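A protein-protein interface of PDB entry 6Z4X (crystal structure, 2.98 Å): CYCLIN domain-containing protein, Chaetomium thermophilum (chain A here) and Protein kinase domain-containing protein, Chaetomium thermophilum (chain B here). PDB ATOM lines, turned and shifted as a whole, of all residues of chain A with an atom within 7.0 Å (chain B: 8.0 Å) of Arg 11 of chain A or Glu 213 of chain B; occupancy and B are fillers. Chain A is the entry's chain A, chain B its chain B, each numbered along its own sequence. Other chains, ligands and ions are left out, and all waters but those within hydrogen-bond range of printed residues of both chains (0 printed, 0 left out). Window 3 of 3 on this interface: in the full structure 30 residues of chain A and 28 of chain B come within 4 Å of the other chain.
O of Trp 210 of chain B lies within hydrogen-bond range of ND2 of Asn 214 of chain B (2.8 Å).
The guanidinium group of Arg 375 of chain B is in salt-bridge range of the side-chain carboxylate of Glu 213 of chain B, at 2.4 Å.
O of Tyr 12 of chain A is in hydrogen-bond range of OG of Ser 15 of chain A.
The side-chain carboxylate of Glu 213 of chain B lies within hydrogen-bond range of the indole nitrogen of Trp 209 of chain B.
Glu 213 of chain B touches just one residue of chain A: Arg 11 (3.4 Å).
No residue of chain B comes within 4 Å of Ala 10 of chain A.
Of the printed residues of chain B, Gln 14 of chain A touches Arg 146 (2.8 Å).
Printed residues of chain B within 4 Å of Ser 15 of chain A: Arg 146.
Printed residues of chain A within 4 Å of Arg 146 of chain B: Gln 14 and Ser 15.
Of the printed residues of chain A, Asn 214 of chain B touches Arg 11 (2.7 Å).
Of the printed residues of chain B, Lys 186 of chain A touches Glu 147.
Ala 374 of chain B touches none of the printed residues of chain A.
Val 208 of chain B touches none of the printed residues of chain A.
The nearest residue of chain B that does not touch Arg 11 of chain A is Trp 210 of chain B (4.3 Å).
The nearest printed residue of chain B that does not touch Lys 186 of chain A is Asn 214 of chain B (6.8 Å).
Of the 18 printed residues of chain B, 4 touch a printed residue of chain A.
O of Glu 213 of chain B lies within hydrogen-bond range of NH2 of Arg 11 of chain A, at 3.4 Å.
NH2 of Arg 11 of chain A sits at hydrogen-bond distance from OD1 of Asn 214 of chain B.
The guanidinium group of Arg 146 of chain B is in hydrogen-bond range of the backbone carbonyl oxygen of Gln 14 of chain A (2.8 Å).
The backbone carbonyl oxygen of Ser 15 of chain A lies close to the guanidinium group of Arg 146 of chain B, 3.4 Å away.
NZ of Lys 186 of chain A lies within salt-bridge range of OE1 of Glu 147 of chain B (3.96 Å).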
ATOM      1  N   ALA A   6      15.597  -4.384  21.832  1.00  0.00           N
ATOM      2  CA  ALA A   6      16.524  -5.490  21.640  1.00  0.00           C
ATOM      3  C   ALA A   6      17.803  -5.008  20.965  1.00  0.00           C
ATOM      4  O   ALA A   6      17.791  -4.100  20.131  1.00  0.00           O
ATOM      5  CB  ALA A   6      15.874  -6.594  20.805  1.00  0.00           C
ATOM      6  N   SER A   7      18.922  -5.634  21.339  1.00  0.00           N
ATOM      7  CA  SER A   7      20.214  -5.227  20.793  1.00  0.00           C
ATOM      8  C   SER A   7      20.327  -5.569  19.311  1.00  0.00           C
ATOM      9  O   SER A   7      20.900  -4.797  18.528  1.00  0.00           O
ATOM     10  CB  SER A   7      21.341  -5.886  21.588  1.00  0.00           C
ATOM     11  OG  SER A   7      21.169  -7.292  21.651  1.00  0.00           O
ATOM     12  N   GLU A   8      19.781  -6.717  18.903  1.00  0.00           N
ATOM     13  CA  GLU A   8      19.814  -7.075  17.490  1.00  0.00           C
ATOM     14  C   GLU A   8      18.987  -6.103  16.658  1.00  0.00           C
ATOM     15  O   GLU A   8      19.374  -5.750  15.536  1.00  0.00           O
ATOM     16  CB  GLU A   8      19.317  -8.509  17.298  1.00  0.00           C
ATOM     17  CG  GLU A   8      17.938  -8.798  17.884  1.00  0.00           C
ATOM     18  CD  GLU A   8      17.998  -9.370  19.291  1.00  0.00           C
ATOM     19  OE1 GLU A   8      18.818  -8.887  20.101  1.00  0.00           O
ATOM     20  OE2 GLU A   8      17.226 -10.310  19.584  1.00  0.00           O
ATOM     21  N   ASP A   9      17.861  -5.637  17.200  1.00  0.00           N
ATOM     22  CA  ASP A   9      17.050  -4.654  16.490  1.00  0.00           C
ATOM     23  C   ASP A   9      17.820  -3.356  16.276  1.00  0.00           C
ATOM     24  O   ASP A   9      17.748  -2.753  15.199  1.00  0.00           O
ATOM     25  CB  ASP A   9      15.754  -4.399  17.259  1.00  0.00           C
ATOM     26  CG  ASP A   9      14.839  -5.611  17.275  1.00  0.00           C
ATOM     27  OD1 ASP A   9      15.149  -6.598  16.574  1.00  0.00           O
ATOM     28  OD2 ASP A   9      13.814  -5.577  17.989  1.00  0.00           O
ATOM     29  N   ALA A  10      18.574  -2.917  17.285  1.00  0.00           N
ATOM     30  CA  ALA A  10      19.385  -1.713  17.132  1.00  0.00           C
ATOM     31  C   ALA A  10      20.478  -1.921  16.092  1.00  0.00           C
ATOM     32  O   ALA A  10      20.689  -1.071  15.215  1.00  0.00           O
ATOM     33  CB  ALA A  10      19.987  -1.311  18.477  1.00  0.00           C
ATOM     34  N   ARG A  11      21.189  -3.051  16.173  1.00  0.00           N
ATOM     35  CA  ARG A  11      22.258  -3.302  15.211  1.00  0.00           C
ATOM     36  C   ARG A  11      21.718  -3.395  13.788  1.00  0.00           C
ATOM     37  O   ARG A  11      22.424  -3.052  12.835  1.00  0.00           O
ATOM     38  CB  ARG A  11      23.033  -4.567  15.592  1.00  0.00           C
ATOM     39  CG  ARG A  11      24.297  -4.794  14.760  1.00  0.00           C
ATOM     40  CD  ARG A  11      25.463  -5.301  15.615  1.00  0.00           C
ATOM     41  NE  ARG A  11      25.411  -6.734  15.905  1.00  0.00           N
ATOM     42  CZ  ARG A  11      26.215  -7.640  15.356  1.00  0.00           C
ATOM     43  NH1 ARG A  11      26.098  -8.919  15.685  1.00  0.00           N
ATOM     44  NH2 ARG A  11      27.138  -7.269  14.479  1.00  0.00           N
ATOM     45  N   TYR A  12      20.470  -3.844  13.622  1.00  0.00           N
ATOM     46  CA  TYR A  12      19.865  -3.818  12.292  1.00  0.00           C
ATOM     47  C   TYR A  12      19.485  -2.400  11.881  1.00  0.00           C
ATOM     48  O   TYR A  12      19.680  -2.011  10.724  1.00  0.00           O
ATOM     49  CB  TYR A  12      18.640  -4.731  12.237  1.00  0.00           C
ATOM     50  CG  TYR A  12      17.946  -4.718  10.891  1.00  0.00           C
ATOM     51  CD1 TYR A  12      18.373  -5.540   9.855  1.00  0.00           C
ATOM     52  CD2 TYR A  12      16.872  -3.874  10.654  1.00  0.00           C
ATOM     53  CE1 TYR A  12      17.744  -5.525   8.623  1.00  0.00           C
ATOM     54  CE2 TYR A  12      16.236  -3.853   9.424  1.00  0.00           C
ATOM     55  CZ  TYR A  12      16.675  -4.680   8.413  1.00  0.00           C
ATOM     56  OH  TYR A  12      16.045  -4.661   7.190  1.00  0.00           O
ATOM     57  N   ARG A  13      18.934  -1.614  12.810  1.00  0.00           N
ATOM     58  CA  ARG A  13      18.605  -0.228  12.496  1.00  0.00           C
ATOM     59  C   ARG A  13      19.843   0.596  12.173  1.00  0.00           C
ATOM     60  O   ARG A  13      19.717   1.681  11.597  1.00  0.00           O
ATOM     61  CB  ARG A  13      17.834   0.417  13.648  1.00  0.00           C
ATOM     62  CG  ARG A  13      16.413  -0.093  13.799  1.00  0.00           C
ATOM     63  CD  ARG A  13      15.623   0.769  14.766  1.00  0.00           C
ATOM     64  NE  ARG A  13      14.374   0.129  15.169  1.00  0.00           N
ATOM     65  CZ  ARG A  13      14.169  -0.421  16.359  1.00  0.00           C
ATOM     66  NH1 ARG A  13      13.002  -0.982  16.641  1.00  0.00           N
ATOM     67  NH2 ARG A  13      15.137  -0.414  17.267  1.00  0.00           N
ATOM     68  N   GLN A  14      21.031   0.113  12.533  1.00  0.00           N
ATOM     69  CA  GLN A  14      22.259   0.811  12.168  1.00  0.00           C
ATOM     70  C   GLN A  14      22.739   0.475  10.760  1.00  0.00           C
ATOM     71  O   GLN A  14      23.713   1.079  10.296  1.00  0.00           O
ATOM     72  CB  GLN A  14      23.373   0.494  13.169  1.00  0.00           C
ATOM     73  CG  GLN A  14      23.072   0.884  14.606  1.00  0.00           C
ATOM     74  CD  GLN A  14      24.311   0.824  15.481  1.00  0.00           C
ATOM     75  OE1 GLN A  14      25.408   1.178  15.046  1.00  0.00           O
ATOM     76  NE2 GLN A  14      24.143   0.370  16.719  1.00  0.00           N
ATOM     77  N   SER A  15      22.085  -0.459  10.072  1.00  0.00           N
ATOM     78  CA  SER A  15      22.531  -0.879   8.754  1.00  0.00           C
ATOM     79  C   SER A  15      22.109   0.132   7.692  1.00  0.00           C
ATOM     80  O   SER A  15      21.153   0.896   7.861  1.00  0.00           O
ATOM     81  CB  SER A  15      21.975  -2.260   8.407  1.00  0.00           C
ATOM     82  OG  SER A  15      20.577  -2.204   8.184  1.00  0.00           O
ATOM     83  N   LYS A 186      21.036  -7.380   2.993  1.00  0.00           N
ATOM     84  CA  LYS A 186      20.776  -8.484   3.907  1.00  0.00           C
ATOM     85  C   LYS A 186      19.612  -9.313   3.384  1.00  0.00           C
ATOM     86  O   LYS A 186      18.550  -8.767   3.066  1.00  0.00           O
ATOM     87  CB  LYS A 186      20.477  -7.963   5.314  1.00  0.00           C
ATOM     88  CG  LYS A 186      21.589  -7.102   5.894  1.00  0.00           C
ATOM     89  CD  LYS A 186      21.207  -6.527   7.243  1.00  0.00           C
ATOM     90  CE  LYS A 186      22.400  -5.863   7.908  1.00  0.00           C
ATOM     91  NZ  LYS A 186      23.529  -6.819   8.083  1.00  0.00           N
ATOM     92  N   ARG B 146      31.167   0.841   5.433  1.00  0.00           N
ATOM     93  CA  ARG B 146      29.815   1.196   5.851  1.00  0.00           C
ATOM     94  C   ARG B 146      29.263   0.179   6.836  1.00  0.00           C
ATOM     95  O   ARG B 146      28.605   0.549   7.816  1.00  0.00           O
ATOM     96  CB  ARG B 146      28.895   1.307   4.635  1.00  0.00           C
ATOM     97  CG  ARG B 146      27.431   1.512   5.000  1.00  0.00           C
ATOM     98  CD  ARG B 146      27.229   2.779   5.814  1.00  0.00           C
ATOM     99  NE  ARG B 146      25.868   2.883   6.333  1.00  0.00           N
ATOM    100  CZ  ARG B 146      25.464   2.336   7.476  1.00  0.00           C
ATOM    101  NH1 ARG B 146      26.316   1.644   8.221  1.00  0.00           N
ATOM    102  NH2 ARG B 146      24.208   2.479   7.876  1.00  0.00           N
ATOM    103  N   GLU B 147      29.527  -1.110   6.603  1.00  0.00           N
ATOM    104  CA  GLU B 147      29.004  -2.126   7.512  1.00  0.00           C
ATOM    105  C   GLU B 147      29.574  -1.972   8.922  1.00  0.00           C
ATOM    106  O   GLU B 147      28.846  -2.117   9.912  1.00  0.00           O
ATOM    107  CB  GLU B 147      29.301  -3.523   6.967  1.00  0.00           C
ATOM    108  CG  GLU B 147      28.333  -3.984   5.890  1.00  0.00           C
ATOM    109  CD  GLU B 147      28.026  -5.469   5.971  1.00  0.00           C
ATOM    110  OE1 GLU B 147      26.838  -5.824   6.146  1.00  0.00           O
ATOM    111  OE2 GLU B 147      28.972  -6.279   5.872  1.00  0.00           O
ATOM    112  N   LEU B 148      30.864  -1.661   9.036  1.00  0.00           N
ATOM    113  CA  LEU B 148      31.535  -1.646  10.331  1.00  0.00           C
ATOM    114  C   LEU B 148      31.561  -0.279  11.004  1.00  0.00           C
ATOM    115  O   LEU B 148      32.004  -0.189  12.155  1.00  0.00           O
ATOM    116  CB  LEU B 148      32.973  -2.153  10.185  1.00  0.00           C
ATOM    117  CG  LEU B 148      33.141  -3.636   9.855  1.00  0.00           C
ATOM    118  CD1 LEU B 148      34.593  -3.955   9.533  1.00  0.00           C
ATOM    119  CD2 LEU B 148      32.644  -4.486  11.012  1.00  0.00           C
ATOM    120  N   ARG B 206      40.487  -5.137  19.602  1.00  0.00           N
ATOM    121  CA  ARG B 206      39.100  -4.687  19.616  1.00  0.00           C
ATOM    122  C   ARG B 206      38.592  -4.441  18.201  1.00  0.00           C
ATOM    123  O   ARG B 206      37.443  -4.770  17.882  1.00  0.00           O
ATOM    124  CB  ARG B 206      38.956  -3.440  20.489  1.00  0.00           C
ATOM    125  CG  ARG B 206      39.045  -3.765  21.967  1.00  0.00           C
ATOM    126  CD  ARG B 206      38.891  -2.557  22.875  1.00  0.00           C
ATOM    127  NE  ARG B 206      38.822  -2.993  24.268  1.00  0.00           N
ATOM    128  CZ  ARG B 206      39.885  -3.227  25.033  1.00  0.00           C
ATOM    129  NH1 ARG B 206      41.105  -3.055  24.541  1.00  0.00           N
ATOM    130  NH2 ARG B 206      39.728  -3.637  26.287  1.00  0.00           N
ATOM    131  N   ALA B 207      39.444  -3.895  17.331  1.00  0.00           N
ATOM    132  CA  ALA B 207      39.044  -3.692  15.942  1.00  0.00           C
ATOM    133  C   ALA B 207      38.737  -5.022  15.261  1.00  0.00           C
ATOM    134  O   ALA B 207      37.711  -5.168  14.583  1.00  0.00           O
ATOM    135  CB  ALA B 207      40.138  -2.936  15.188  1.00  0.00           C
ATOM    136  N   VAL B 208      39.620  -6.008  15.428  1.00  0.00           N
ATOM    137  CA  VAL B 208      39.397  -7.304  14.789  1.00  0.00           C
ATOM    138  C   VAL B 208      38.186  -8.005  15.399  1.00  0.00           C
ATOM    139  O   VAL B 208      37.442  -8.705  14.700  1.00  0.00           O
ATOM    140  CB  VAL B 208      40.659  -8.178  14.873  1.00  0.00           C
ATOM    141  CG1 VAL B 208      40.373  -9.559  14.310  1.00  0.00           C
ATOM    142  CG2 VAL B 208      41.799  -7.522  14.109  1.00  0.00           C
ATOM    143  N   TRP B 209      37.979  -7.849  16.709  1.00  0.00           N
ATOM    144  CA  TRP B 209      36.801  -8.435  17.336  1.00  0.00           C
ATOM    145  C   TRP B 209      35.530  -7.828  16.771  1.00  0.00           C
ATOM    146  O   TRP B 209      34.546  -8.537  16.540  1.00  0.00           O
ATOM    147  CB  TRP B 209      36.843  -8.253  18.853  1.00  0.00           C
ATOM    148  CG  TRP B 209      35.518  -8.556  19.492  1.00  0.00           C
ATOM    149  CD1 TRP B 209      35.049  -9.782  19.859  1.00  0.00           C
ATOM    150  CD2 TRP B 209      34.484  -7.617  19.815  1.00  0.00           C
ATOM    151  NE1 TRP B 209      33.791  -9.666  20.398  1.00  0.00           N
ATOM    152  CE2 TRP B 209      33.421  -8.347  20.382  1.00  0.00           C
ATOM    153  CE3 TRP B 209      34.355  -6.232  19.681  1.00  0.00           C
ATOM    154  CZ2 TRP B 209      32.245  -7.739  20.816  1.00  0.00           C
ATOM    155  CZ3 TRP B 209      33.186  -5.630  20.114  1.00  0.00           C
ATOM    156  CH2 TRP B 209      32.147  -6.383  20.675  1.00  0.00           C
ATOM    157  N   TRP B 210      35.522  -6.510  16.558  1.00  0.00           N
ATOM    158  CA  TRP B 210      34.352  -5.876  15.961  1.00  0.00           C
ATOM    159  C   TRP B 210      34.152  -6.351  14.527  1.00  0.00           C
ATOM    160  O   TRP B 210      33.013  -6.556  14.087  1.00  0.00           O
ATOM    161  CB  TRP B 210      34.487  -4.357  16.030  1.00  0.00           C
ATOM    162  CG  TRP B 210      33.289  -3.628  15.514  1.00  0.00           C
ATOM    163  CD1 TRP B 210      33.253  -2.749  14.472  1.00  0.00           C
ATOM    164  CD2 TRP B 210      31.943  -3.728  16.001  1.00  0.00           C
ATOM    165  NE1 TRP B 210      31.973  -2.282  14.289  1.00  0.00           N
ATOM    166  CE2 TRP B 210      31.149  -2.870  15.213  1.00  0.00           C
ATOM    167  CE3 TRP B 210      31.333  -4.458  17.028  1.00  0.00           C
ATOM    168  CZ2 TRP B 210      29.779  -2.719  15.420  1.00  0.00           C
ATOM    169  CZ3 TRP B 210      29.970  -4.306  17.232  1.00  0.00           C
ATOM    170  CH2 TRP B 210      29.210  -3.444  16.431  1.00  0.00           C
ATOM    171  N   CYS B 211      35.247  -6.532  13.786  1.00  0.00           N
ATOM    172  CA  CYS B 211      35.152  -7.097  12.444  1.00  0.00           C
ATOM    173  C   CYS B 211      34.453  -8.453  12.473  1.00  0.00           C
ATOM    174  O   CYS B 211      33.436  -8.660  11.800  1.00  0.00           O
ATOM    175  CB  CYS B 211      36.547  -7.225  11.826  1.00  0.00           C
ATOM    176  SG  CYS B 211      37.280  -5.686  11.248  1.00  0.00           S
ATOM    177  N   HIS B 212      34.989  -9.390  13.261  1.00  0.00           N
ATOM    178  CA  HIS B 212      34.448 -10.749  13.268  1.00  0.00           C
ATOM    179  C   HIS B 212      33.046 -10.802  13.864  1.00  0.00           C
ATOM    180  O   HIS B 212      32.222 -11.619  13.435  1.00  0.00           O
ATOM    181  CB  HIS B 212      35.391 -11.684  14.027  1.00  0.00           C
ATOM    182  CG  HIS B 212      36.713 -11.888  13.351  1.00  0.00           C
ATOM    183  ND1 HIS B 212      37.730 -12.628  13.916  1.00  0.00           N
ATOM    184  CD2 HIS B 212      37.179 -11.463  12.153  1.00  0.00           C
ATOM    185  CE1 HIS B 212      38.770 -12.638  13.101  1.00  0.00           C
ATOM    186  NE2 HIS B 212      38.461 -11.940  12.023  1.00  0.00           N
ATOM    187  N   GLU B 213      32.751  -9.934  14.836  1.00  0.00           N
ATOM    188  CA  GLU B 213      31.411  -9.876  15.405  1.00  0.00           C
ATOM    189  C   GLU B 213      30.370  -9.575  14.339  1.00  0.00           C
ATOM    190  O   GLU B 213      29.213  -9.991  14.464  1.00  0.00           O
ATOM    191  CB  GLU B 213      31.361  -8.818  16.511  1.00  0.00           C
ATOM    192  CG  GLU B 213      30.256  -9.025  17.538  1.00  0.00           C
ATOM    193  CD  GLU B 213      30.478 -10.252  18.397  1.00  0.00           C
ATOM    194  OE1 GLU B 213      29.479 -10.853  18.848  1.00  0.00           O
ATOM    195  OE2 GLU B 213      31.651 -10.626  18.611  1.00  0.00           O
ATOM    196  N   ASN B 214      30.761  -8.856  13.287  1.00  0.00           N
ATOM    197  CA  ASN B 214      29.888  -8.562  12.160  1.00  0.00           C
ATOM    198  C   ASN B 214      30.163  -9.467  10.966  1.00  0.00           C
ATOM    199  O   ASN B 214      29.721  -9.167   9.852  1.00  0.00           O
ATOM    200  CB  ASN B 214      30.023  -7.093  11.757  1.00  0.00           C
ATOM    201  CG  ASN B 214      29.482  -6.149  12.813  1.00  0.00           C
ATOM    202  OD1 ASN B 214      28.346  -5.685  12.720  1.00  0.00           O
ATOM    203  ND2 ASN B 214      30.289  -5.868  13.832  1.00  0.00           N
ATOM    204  N   PHE B 215      30.880 -10.571  11.176  1.00  0.00           N
ATOM    205  CA  PHE B 215      31.089 -11.581  10.141  1.00  0.00           C
ATOM    206  C   PHE B 215      31.818 -10.990   8.934  1.00  0.00           C
ATOM    207  O   PHE B 215      31.348 -11.040   7.795  1.00  0.00           O
ATOM    208  CB  PHE B 215      29.755 -12.206   9.733  1.00  0.00           C
ATOM    209  CG  PHE B 215      28.859 -12.501  10.892  1.00  0.00           C
ATOM    210  CD1 PHE B 215      29.140 -13.551  11.748  1.00  0.00           C
ATOM    211  CD2 PHE B 215      27.743 -11.719  11.138  1.00  0.00           C
ATOM    212  CE1 PHE B 215      28.320 -13.824  12.823  1.00  0.00           C
ATOM    213  CE2 PHE B 215      26.916 -11.986  12.211  1.00  0.00           C
ATOM    214  CZ  PHE B 215      27.205 -13.041  13.056  1.00  0.00           C
ATOM    215  N   ILE B 216      32.990 -10.423   9.206  1.00  0.00           N
ATOM    216  CA  ILE B 216      33.834  -9.851   8.166  1.00  0.00           C
ATOM    217  C   ILE B 216      35.276 -10.238   8.454  1.00  0.00           C
ATOM    218  O   ILE B 216      35.765 -10.045   9.573  1.00  0.00           O
ATOM    219  CB  ILE B 216      33.696  -8.317   8.096  1.00  0.00           C
ATOM    220  CG1 ILE B 216      32.251  -7.926   7.785  1.00  0.00           C
ATOM    221  CG2 ILE B 216      34.649  -7.746   7.052  1.00  0.00           C
ATOM    222  CD1 ILE B 216      31.966  -6.449   7.966  1.00  0.00           C
ATOM    223  N   PHE B 245      32.007 -13.658   5.973  1.00  0.00           N
ATOM    224  CA  PHE B 245      32.149 -15.060   6.343  1.00  0.00           C
ATOM    225  C   PHE B 245      31.436 -15.941   5.323  1.00  0.00           C
ATOM    226  O   PHE B 245      30.227 -15.803   5.105  1.00  0.00           O
ATOM    227  CB  PHE B 245      31.586 -15.298   7.744  1.00  0.00           C
ATOM    228  CG  PHE B 245      32.434 -14.729   8.852  1.00  0.00           C
ATOM    229  CD1 PHE B 245      33.537 -13.935   8.573  1.00  0.00           C
ATOM    230  CD2 PHE B 245      32.125 -14.994  10.177  1.00  0.00           C
ATOM    231  CE1 PHE B 245      34.308 -13.411   9.598  1.00  0.00           C
ATOM    232  CE2 PHE B 245      32.894 -14.476  11.204  1.00  0.00           C
ATOM    233  CZ  PHE B 245      33.986 -13.684  10.914  1.00  0.00           C
ATOM    234  N   ALA B 374      39.141 -13.800  18.700  1.00  0.00           N
ATOM    235  CA  ALA B 374      39.201 -12.399  19.105  1.00  0.00           C
ATOM    236  C   ALA B 374      38.480 -12.168  20.427  1.00  0.00           C
ATOM    237  O   ALA B 374      38.955 -11.403  21.276  1.00  0.00           O
ATOM    238  CB  ALA B 374      38.614 -11.511  18.010  1.00  0.00           C
ATOM    239  N   ARG B 375      37.331 -12.820  20.620  1.00  0.00           N
ATOM    240  CA  ARG B 375      36.634 -12.716  21.897  1.00  0.00           C
ATOM    241  C   ARG B 375      37.474 -13.310  23.019  1.00  0.00           C
ATOM    242  O   ARG B 375      37.698 -12.666  24.052  1.00  0.00           O
ATOM    243  CB  ARG B 375      35.272 -13.404  21.815  1.00  0.00           C
ATOM    244  CG  ARG B 375      34.346 -13.057  22.969  1.00  0.00           C
ATOM    245  CD  ARG B 375      32.965 -13.641  22.753  1.00  0.00           C
ATOM    246  NE  ARG B 375      32.234 -12.916  21.717  1.00  0.00           N
ATOM    247  CZ  ARG B 375      30.961 -13.138  21.408  1.00  0.00           C
ATOM    248  NH1 ARG B 375      30.277 -14.073  22.053  1.00  0.00           N
ATOM    249  NH2 ARG B 375      30.376 -12.435  20.449  1.00  0.00           N
ATOM    250  N   LEU B 378      40.240 -10.827  23.834  1.00  0.00           N
ATOM    251  CA  LEU B 378      39.884  -9.693  24.679  1.00  0.00           C
ATOM    252  C   LEU B 378      39.674 -10.102  26.130  1.00  0.00           C
ATOM    253  O   LEU B 378      39.734  -9.244  27.019  1.00  0.00           O
ATOM    254  CB  LEU B 378      38.625  -8.998  24.154  1.00  0.00           C
ATOM    255  CG  LEU B 378      38.787  -8.139  22.899  1.00  0.00           C
ATOM    256  CD1 LEU B 378      37.440  -7.620  22.421  1.00  0.00           C
ATOM    257  CD2 LEU B 378      39.737  -6.984  23.179  1.00  0.00           C
